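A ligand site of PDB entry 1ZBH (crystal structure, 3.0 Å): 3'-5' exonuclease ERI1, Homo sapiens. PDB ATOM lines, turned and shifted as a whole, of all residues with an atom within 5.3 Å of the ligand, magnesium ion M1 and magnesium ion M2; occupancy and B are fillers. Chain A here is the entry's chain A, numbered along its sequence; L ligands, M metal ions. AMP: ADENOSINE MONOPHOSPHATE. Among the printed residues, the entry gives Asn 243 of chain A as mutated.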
ATOM      1  N   ASP A  84     -21.321  14.378   1.251  1.00  0.00           N
ATOM      2  CA  ASP A  84     -20.070  14.096   1.959  1.00  0.00           C
ATOM      3  C   ASP A  84     -18.993  13.559   1.035  1.00  0.00           C
ATOM      4  O   ASP A  84     -18.891  12.351   0.797  1.00  0.00           O
ATOM      5  CB  ASP A  84     -20.293  13.148   3.144  1.00  0.00           C
ATOM      6  CG  ASP A  84     -19.079  13.087   4.049  1.00  0.00           C
ATOM      7  OD1 ASP A  84     -18.538  14.165   4.403  1.00  0.00           O
ATOM      8  OD2 ASP A  84     -18.656  11.969   4.417  1.00  0.00           O
ATOM      9  N   PHE A  85     -18.165  14.465   0.530  1.00  0.00           N
ATOM     10  CA  PHE A  85     -17.101  14.117  -0.409  1.00  0.00           C
ATOM     11  C   PHE A  85     -16.097  13.172   0.223  1.00  0.00           C
ATOM     12  O   PHE A  85     -15.805  13.248   1.426  1.00  0.00           O
ATOM     13  CB  PHE A  85     -16.346  15.361  -0.882  1.00  0.00           C
ATOM     14  CG  PHE A  85     -17.208  16.360  -1.602  1.00  0.00           C
ATOM     15  CD1 PHE A  85     -17.884  16.000  -2.764  1.00  0.00           C
ATOM     16  CD2 PHE A  85     -17.317  17.652  -1.130  1.00  0.00           C
ATOM     17  CE1 PHE A  85     -18.681  16.916  -3.440  1.00  0.00           C
ATOM     18  CE2 PHE A  85     -18.108  18.589  -1.799  1.00  0.00           C
ATOM     19  CZ  PHE A  85     -18.785  18.221  -2.950  1.00  0.00           C
ATOM     20  N   GLU A  86     -15.586  12.271  -0.603  1.00  0.00           N
ATOM     21  CA  GLU A  86     -14.350  11.582  -0.324  1.00  0.00           C
ATOM     22  C   GLU A  86     -13.343  12.094  -1.328  1.00  0.00           C
ATOM     23  O   GLU A  86     -13.702  12.402  -2.465  1.00  0.00           O
ATOM     24  CB  GLU A  86     -14.506  10.064  -0.433  1.00  0.00           C
ATOM     25  CG  GLU A  86     -15.477   9.451   0.580  1.00  0.00           C
ATOM     26  CD  GLU A  86     -15.146   9.780   2.027  1.00  0.00           C
ATOM     27  OE1 GLU A  86     -14.019   9.475   2.490  1.00  0.00           O
ATOM     28  OE2 GLU A  86     -16.035  10.325   2.731  1.00  0.00           O
ATOM     29  N   ALA A  87     -12.088  12.201  -0.900  1.00  0.00           N
ATOM     30  CA  ALA A  87     -11.028  12.737  -1.751  1.00  0.00           C
ATOM     31  C   ALA A  87      -9.735  11.946  -1.556  1.00  0.00           C
ATOM     32  O   ALA A  87      -9.563  11.288  -0.538  1.00  0.00           O
ATOM     33  CB  ALA A  87     -10.803  14.210  -1.441  1.00  0.00           C
ATOM     34  N   THR A  88      -8.852  12.030  -2.553  1.00  0.00           N
ATOM     35  CA  THR A  88      -7.526  11.406  -2.489  1.00  0.00           C
ATOM     36  C   THR A  88      -6.752  11.878  -1.264  1.00  0.00           C
ATOM     37  O   THR A  88      -6.839  13.045  -0.879  1.00  0.00           O
ATOM     38  CB  THR A  88      -6.686  11.694  -3.754  1.00  0.00           C
ATOM     39  OG1 THR A  88      -6.542  13.113  -3.925  1.00  0.00           O
ATOM     40  CG2 THR A  88      -7.327  11.103  -4.990  1.00  0.00           C
ATOM     41  N   CYS A  89      -5.999  10.973  -0.645  1.00  0.00           N
ATOM     42  CA  CYS A  89      -5.199  11.285   0.538  1.00  0.00           C
ATOM     43  C   CYS A  89      -4.064  10.290   0.721  1.00  0.00           C
ATOM     44  O   CYS A  89      -4.121   9.176   0.195  1.00  0.00           O
ATOM     45  CB  CYS A  89      -6.090  11.277   1.780  1.00  0.00           C
ATOM     46  SG  CYS A  89      -6.927   9.709   2.075  1.00  0.00           S
ATOM     47  N   GLU A  90      -3.032  10.696   1.462  1.00  0.00           N
ATOM     48  CA  GLU A  90      -1.943   9.811   1.840  1.00  0.00           C
ATOM     49  C   GLU A  90      -1.903   9.575   3.346  1.00  0.00           C
ATOM     50  O   GLU A  90      -2.495  10.351   4.120  1.00  0.00           O
ATOM     51  CB  GLU A  90      -0.593  10.363   1.376  1.00  0.00           C
ATOM     52  CG  GLU A  90       0.019   9.615   0.198  1.00  0.00           C
ATOM     53  CD  GLU A  90      -0.418  10.169  -1.137  1.00  0.00           C
ATOM     54  OE1 GLU A  90      -1.631  10.103  -1.454  1.00  0.00           O
ATOM     55  OE2 GLU A  90       0.446  10.678  -1.886  1.00  0.00           O
ATOM     56  N   GLY A  92      -0.991   9.709   7.056  1.00  0.00           N
ATOM     57  CA  GLY A  92      -0.461  10.763   7.915  1.00  0.00           C
ATOM     58  C   GLY A  92      -0.812  12.174   7.475  1.00  0.00           C
ATOM     59  O   GLY A  92      -0.302  13.140   8.043  1.00  0.00           O
ATOM     60  N   ASN A  93      -1.690  12.281   6.477  1.00  0.00           N
ATOM     61  CA  ASN A  93      -2.199  13.554   5.976  1.00  0.00           C
ATOM     62  C   ASN A  93      -1.095  14.597   5.689  1.00  0.00           C
ATOM     63  O   ASN A  93      -0.997  15.599   6.409  1.00  0.00           O
ATOM     64  CB  ASN A  93      -3.230  14.123   6.971  1.00  0.00           C
ATOM     65  CG  ASN A  93      -4.272  15.010   6.311  1.00  0.00           C
ATOM     66  OD1 ASN A  93      -4.941  14.602   5.359  1.00  0.00           O
ATOM     67  ND2 ASN A  93      -4.440  16.213   6.845  1.00  0.00           N
ATOM     68  N   HIS A  99      -5.406  17.656  -3.004  1.00  0.00           N
ATOM     69  CA  HIS A  99      -6.593  16.818  -2.858  1.00  0.00           C
ATOM     70  C   HIS A  99      -7.480  16.862  -4.100  1.00  0.00           C
ATOM     71  O   HIS A  99      -7.605  17.910  -4.743  1.00  0.00           O
ATOM     72  CB  HIS A  99      -7.399  17.255  -1.640  1.00  0.00           C
ATOM     73  CG  HIS A  99      -6.763  16.909  -0.331  1.00  0.00           C
ATOM     74  ND1 HIS A  99      -6.602  15.606   0.099  1.00  0.00           N
ATOM     75  CD2 HIS A  99      -6.253  17.686   0.651  1.00  0.00           C
ATOM     76  CE1 HIS A  99      -6.020  15.606   1.284  1.00  0.00           C
ATOM     77  NE2 HIS A  99      -5.797  16.857   1.636  1.00  0.00           N
ATOM     78  N   PHE A 135      -3.152   3.819   1.493  1.00  0.00           N
ATOM     79  CA  PHE A 135      -3.875   4.310   2.661  1.00  0.00           C
ATOM     80  C   PHE A 135      -5.271   4.789   2.270  1.00  0.00           C
ATOM     81  O   PHE A 135      -6.256   4.476   2.947  1.00  0.00           O
ATOM     82  CB  PHE A 135      -3.089   5.455   3.329  1.00  0.00           C
ATOM     83  CG  PHE A 135      -3.842   6.179   4.407  1.00  0.00           C
ATOM     84  CD1 PHE A 135      -3.880   5.686   5.706  1.00  0.00           C
ATOM     85  CD2 PHE A 135      -4.505   7.374   4.132  1.00  0.00           C
ATOM     86  CE1 PHE A 135      -4.568   6.369   6.709  1.00  0.00           C
ATOM     87  CE2 PHE A 135      -5.192   8.066   5.124  1.00  0.00           C
ATOM     88  CZ  PHE A 135      -5.225   7.551   6.425  1.00  0.00           C
ATOM     89  N   LEU A 139      -8.832   3.476   3.588  1.00  0.00           N
ATOM     90  CA  LEU A 139      -9.716   4.325   4.360  1.00  0.00           C
ATOM     91  C   LEU A 139     -11.105   4.407   3.740  1.00  0.00           C
ATOM     92  O   LEU A 139     -12.085   3.951   4.334  1.00  0.00           O
ATOM     93  CB  LEU A 139      -9.127   5.733   4.518  1.00  0.00           C
ATOM     94  CG  LEU A 139      -9.919   6.748   5.356  1.00  0.00           C
ATOM     95  CD1 LEU A 139      -9.683   6.513   6.845  1.00  0.00           C
ATOM     96  CD2 LEU A 139      -9.547   8.165   4.961  1.00  0.00           C
ATOM     97  N   THR A 140     -11.175   4.965   2.539  1.00  0.00           N
ATOM     98  CA  THR A 140     -12.431   5.228   1.834  1.00  0.00           C
ATOM     99  C   THR A 140     -13.153   3.977   1.366  1.00  0.00           C
ATOM    100  O   THR A 140     -14.384   3.970   1.236  1.00  0.00           O
ATOM    101  CB  THR A 140     -12.208   6.115   0.597  1.00  0.00           C
ATOM    102  OG1 THR A 140     -11.279   5.476  -0.282  1.00  0.00           O
ATOM    103  CG2 THR A 140     -11.670   7.483   0.992  1.00  0.00           C
ATOM    104  N   ASP A 180     -20.875  17.211   7.207  1.00  0.00           N
ATOM    105  CA  ASP A 180     -20.182  16.978   8.472  1.00  0.00           C
ATOM    106  C   ASP A 180     -18.843  17.703   8.494  1.00  0.00           C
ATOM    107  O   ASP A 180     -17.858  17.247   7.897  1.00  0.00           O
ATOM    108  CB  ASP A 180     -19.976  15.477   8.730  1.00  0.00           C
ATOM    109  CG  ASP A 180     -19.209  15.199  10.022  1.00  0.00           C
ATOM    110  OD1 ASP A 180     -19.482  15.874  11.032  1.00  0.00           O
ATOM    111  OD2 ASP A 180     -18.335  14.309  10.011  1.00  0.00           O
ATOM    112  N   TRP A 183     -14.833  21.168   5.963  1.00  0.00           N
ATOM    113  CA  TRP A 183     -13.965  20.583   4.941  1.00  0.00           C
ATOM    114  C   TRP A 183     -14.618  20.428   3.553  1.00  0.00           C
ATOM    115  O   TRP A 183     -14.099  20.938   2.555  1.00  0.00           O
ATOM    116  CB  TRP A 183     -13.428  19.227   5.430  1.00  0.00           C
ATOM    117  CG  TRP A 183     -12.086  19.336   6.110  1.00  0.00           C
ATOM    118  CD1 TRP A 183     -11.461  20.476   6.526  1.00  0.00           C
ATOM    119  CD2 TRP A 183     -11.222  18.241   6.467  1.00  0.00           C
ATOM    120  NE1 TRP A 183     -10.249  20.171   7.110  1.00  0.00           N
ATOM    121  CE2 TRP A 183     -10.075  18.806   7.088  1.00  0.00           C
ATOM    122  CE3 TRP A 183     -11.285  16.850   6.317  1.00  0.00           C
ATOM    123  CZ2 TRP A 183      -9.012  18.027   7.556  1.00  0.00           C
ATOM    124  CZ3 TRP A 183     -10.234  16.063   6.788  1.00  0.00           C
ATOM    125  CH2 TRP A 183      -9.110  16.665   7.407  1.00  0.00           C
ATOM    126  N   ASP A 184     -15.759  19.754   3.507  1.00  0.00           N
ATOM    127  CA  ASP A 184     -16.402  19.398   2.238  1.00  0.00           C
ATOM    128  C   ASP A 184     -16.415  20.537   1.211  1.00  0.00           C
ATOM    129  O   ASP A 184     -15.869  20.406   0.117  1.00  0.00           O
ATOM    130  CB  ASP A 184     -17.804  18.842   2.495  1.00  0.00           C
ATOM    131  CG  ASP A 184     -17.773  17.411   3.022  1.00  0.00           C
ATOM    132  OD1 ASP A 184     -18.515  16.580   2.476  1.00  0.00           O
ATOM    133  OD2 ASP A 184     -17.012  17.116   3.970  1.00  0.00           O
ATOM    134  N   PHE A 188     -12.393  20.709   0.065  1.00  0.00           N
ATOM    135  CA  PHE A 188     -12.433  19.758  -1.057  1.00  0.00           C
ATOM    136  C   PHE A 188     -12.999  20.321  -2.345  1.00  0.00           C
ATOM    137  O   PHE A 188     -12.354  20.269  -3.382  1.00  0.00           O
ATOM    138  CB  PHE A 188     -13.127  18.455  -0.655  1.00  0.00           C
ATOM    139  CG  PHE A 188     -12.419  17.710   0.457  1.00  0.00           C
ATOM    140  CD1 PHE A 188     -11.056  17.402   0.348  1.00  0.00           C
ATOM    141  CD2 PHE A 188     -13.107  17.331   1.602  1.00  0.00           C
ATOM    142  CE1 PHE A 188     -10.397  16.739   1.374  1.00  0.00           C
ATOM    143  CE2 PHE A 188     -12.462  16.651   2.631  1.00  0.00           C
ATOM    144  CZ  PHE A 188     -11.095  16.362   2.520  1.00  0.00           C
ATOM    145  N   ARG A 211     -21.861  19.919  12.679  1.00  0.00           N
ATOM    146  CA  ARG A 211     -21.038  19.876  13.899  1.00  0.00           C
ATOM    147  C   ARG A 211     -21.249  21.107  14.771  1.00  0.00           C
ATOM    148  O   ARG A 211     -21.347  21.002  15.991  1.00  0.00           O
ATOM    149  CB  ARG A 211     -19.556  19.748  13.556  1.00  0.00           C
ATOM    150  CG  ARG A 211     -19.158  18.344  13.163  1.00  0.00           C
ATOM    151  CD  ARG A 211     -17.705  18.246  12.768  1.00  0.00           C
ATOM    152  NE  ARG A 211     -17.344  16.860  12.479  1.00  0.00           N
ATOM    153  CZ  ARG A 211     -16.348  16.480  11.676  1.00  0.00           C
ATOM    154  NH1 ARG A 211     -15.590  17.395  11.067  1.00  0.00           N
ATOM    155  NH2 ARG A 211     -16.117  15.195  11.482  1.00  0.00           N
ATOM    156  N   ASN A 243     -16.428   5.746   6.505  1.00  0.00           N
ATOM    157  CA  ASN A 243     -15.583   6.459   5.525  1.00  0.00           C
ATOM    158  C   ASN A 243     -15.995   6.303   4.054  1.00  0.00           C
ATOM    159  O   ASN A 243     -15.368   6.868   3.166  1.00  0.00           O
ATOM    160  CB  ASN A 243     -14.085   6.153   5.735  1.00  0.00           C
ATOM    161  CG  ASN A 243     -13.597   6.547   7.121  1.00  0.00           C
ATOM    162  OD1 ASN A 243     -12.861   5.807   7.760  1.00  0.00           O
ATOM    163  ND2 ASN A 243     -14.008   7.725   7.579  1.00  0.00           N
ATOM    164  N   CYS A 244     -17.063   5.537   3.828  1.00  0.00           N
ATOM    165  CA  CYS A 244     -17.672   5.446   2.506  1.00  0.00           C
ATOM    166  C   CYS A 244     -18.651   6.618   2.368  1.00  0.00           C
ATOM    167  O   CYS A 244     -19.657   6.681   3.075  1.00  0.00           O
ATOM    168  CB  CYS A 244     -18.361   4.094   2.344  1.00  0.00           C
ATOM    169  SG  CYS A 244     -19.768   4.017   1.219  1.00  0.00           S
ATOM    170  N   GLY A 245     -18.322   7.548   1.468  1.00  0.00           N
ATOM    171  CA  GLY A 245     -19.050   8.818   1.292  1.00  0.00           C
ATOM    172  C   GLY A 245     -20.563   8.763   1.381  1.00  0.00           C
ATOM    173  O   GLY A 245     -21.164   9.501   2.161  1.00  0.00           O
ATOM    174  N   ASP A 248     -21.649   7.515   4.803  1.00  0.00           N
ATOM    175  CA  ASP A 248     -21.443   8.619   5.718  1.00  0.00           C
ATOM    176  C   ASP A 248     -22.620   9.577   5.627  1.00  0.00           C
ATOM    177  O   ASP A 248     -23.281   9.856   6.624  1.00  0.00           O
ATOM    178  CB  ASP A 248     -20.142   9.358   5.407  1.00  0.00           C
ATOM    179  CG  ASP A 248     -18.897   8.583   5.809  1.00  0.00           C
ATOM    180  OD1 ASP A 248     -17.987   8.479   4.968  1.00  0.00           O
ATOM    181  OD2 ASP A 248     -18.813   8.096   6.958  1.00  0.00           O
ATOM    182  N   ILE A 252     -25.116  10.813   8.557  1.00  0.00           N
ATOM    183  CA  ILE A 252     -25.258  12.246   8.830  1.00  0.00           C
ATOM    184  C   ILE A 252     -26.733  12.639   8.728  1.00  0.00           C
ATOM    185  O   ILE A 252     -27.225  13.419   9.548  1.00  0.00           O
ATOM    186  CB  ILE A 252     -24.383  13.103   7.877  1.00  0.00           C
ATOM    187  CG1 ILE A 252     -22.910  12.701   7.981  1.00  0.00           C
ATOM    188  CG2 ILE A 252     -24.528  14.586   8.194  1.00  0.00           C
ATOM    189  CD1 ILE A 252     -22.079  13.095   6.774  1.00  0.00           C
HETATM  190  P   AMP L   1     -14.868  12.390   5.774  1.00  0.00           P
HETATM  191  O1P AMP L   1     -15.914  13.126   4.964  1.00  0.00           O
HETATM  192  O2P AMP L   1     -14.950  10.877   5.675  1.00  0.00           O
HETATM  193  O3P AMP L   1     -14.686  12.924   7.161  1.00  0.00           O
HETATM  194  O5' AMP L   1     -13.473  12.739   5.048  1.00  0.00           O
HETATM  195  C5' AMP L   1     -13.323  12.477   3.659  1.00  0.00           C
HETATM  196  C4' AMP L   1     -11.927  12.783   3.163  1.00  0.00           C
HETATM  197  O4' AMP L   1     -11.095  13.399   4.156  1.00  0.00           O
HETATM  198  C3' AMP L   1     -11.215  11.516   2.739  1.00  0.00           C
HETATM  199  O3' AMP L   1     -11.459  11.210   1.369  1.00  0.00           O
HETATM  200  C2' AMP L   1      -9.756  11.831   2.977  1.00  0.00           C
HETATM  201  O2' AMP L   1      -9.160  12.383   1.799  1.00  0.00           O
HETATM  202  C1' AMP L   1      -9.769  12.858   4.096  1.00  0.00           C
HETATM  203  N9  AMP L   1      -9.426  12.169   5.361  1.00  0.00           N
HETATM  204  C8  AMP L   1     -10.315  11.773   6.301  1.00  0.00           C
HETATM  205  N7  AMP L   1      -9.690  11.172   7.342  1.00  0.00           N
HETATM  206  C5  AMP L   1      -8.374  11.172   7.074  1.00  0.00           C
HETATM  207  C6  AMP L   1      -7.157  10.696   7.763  1.00  0.00           C
HETATM  208  N6  AMP L   1      -7.247  10.084   8.963  1.00  0.00           N
HETATM  209  N1  AMP L   1      -5.957  10.894   7.146  1.00  0.00           N
HETATM  210  C2  AMP L   1      -5.867  11.507   5.946  1.00  0.00           C
HETATM  211  N3  AMP L   1      -6.945  11.959   5.262  1.00  0.00           N
HETATM  212  C4  AMP L   1      -8.200  11.828   5.765  1.00  0.00           C
HETATM  213 MG    MG M   1     -16.987  14.102   6.008  1.00  0.00          MG
HETATM  214 MG    MG M   2     -17.003  10.740   4.595  1.00  0.00          MG
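Magnesium ion M2 is bound by OD2 of Asp 84, 2.1 Å away.
OE2 of Glu 86 is bound to magnesium ion M2 (2.1 Å).
O2P of the ligand binds magnesium ion M2 (2.3 Å).
Magnesium ion M2 is bound by OD1 of Asp 248 (2.5 Å).
Magnesium ion M2 has four donor atoms within binding distance.
Slightly farther from magnesium ion M2 lies an oxygen (O1P) of the ligand (2.6 Å).
Merely in contact with the ligand: Phe 85 (3.4 Å), Thr 88 (3.6 Å), Phe 135 (3.5 Å), Leu 139 (3.8 Å), Thr 140 (3.8 Å), Trp 183 (3.8 Å), Phe 188 (3.4 Å) and Asn 243 (3.8 Å).
Hydrophobic or aromatic side chains that line the ligand: Phe 135, Leu 139, Trp 183 and Phe 188.
The nearest printed residue that does not touch the ligand is Glu 90 (4.01 Å).
The side-chain carboxylate (OD2) of Asp 248 sits at hydrogen-bond distance from the backbone NH (N) of Asn 243, at 3.4 Å.
OD1 of Asp 248 sits close to N of Cys 244 (3.3 Å).
The backbone NH of Phe 188 lies within hydrogen-bond range of the backbone carbonyl oxygen of Trp 183 (3.0 Å).
The backbone NH of Phe 85 lies within hydrogen-bond range of the side-chain carboxylate of Asp 184, 2.9 Å away.
The backbone carbonyl oxygen (O) of Thr 88 lies within hydrogen-bond range of a ring nitrogen (ND1) of His 99 (2.8 Å).
OD1 of Asp 180 lies within salt-bridge range of NE of Arg 211.
N of Ala 87 sits at hydrogen-bond distance from O3' of the ligand, at 2.6 Å.
The backbone carbonyl oxygen of Ala 87 lies within hydrogen-bond range of an oxygen (O2') of the ligand (2.6 Å).
O2' of the ligand sits close to SG of Cys 89 (3.5 Å).
The side-chain amide oxygen of Asn 93 sits close to a nitrogen (N3) of the ligand, at 3.3 Å.
Residues that only touch magnesium ion M1: Asp 184 (3.6 Å) and Asp 180 (3.8 Å).
Of the 23 residues printed, 3 come within 4 Å of magnesium ion M1.
The nearest printed residue that does not touch magnesium ion M1 is Phe 85 (4.8 Å).
Magnesium ion M1 is bound by an oxygen (O1P) of the ligand (1.8 Å) and the side-chain carboxylate of Asp 84 (2.2 Å).
Slightly farther from magnesium ion M1 lies O3P of the ligand (2.8 Å).
Within 4 Å of magnesium ion M2: Asp 84, Glu 86 and Asp 248.
Along chain A the residues within 4 Å of magnesium ion M2 span positions 84 to 248.
The nearest printed residue that does not touch magnesium ion M2 is Phe 85 (4.2 Å).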
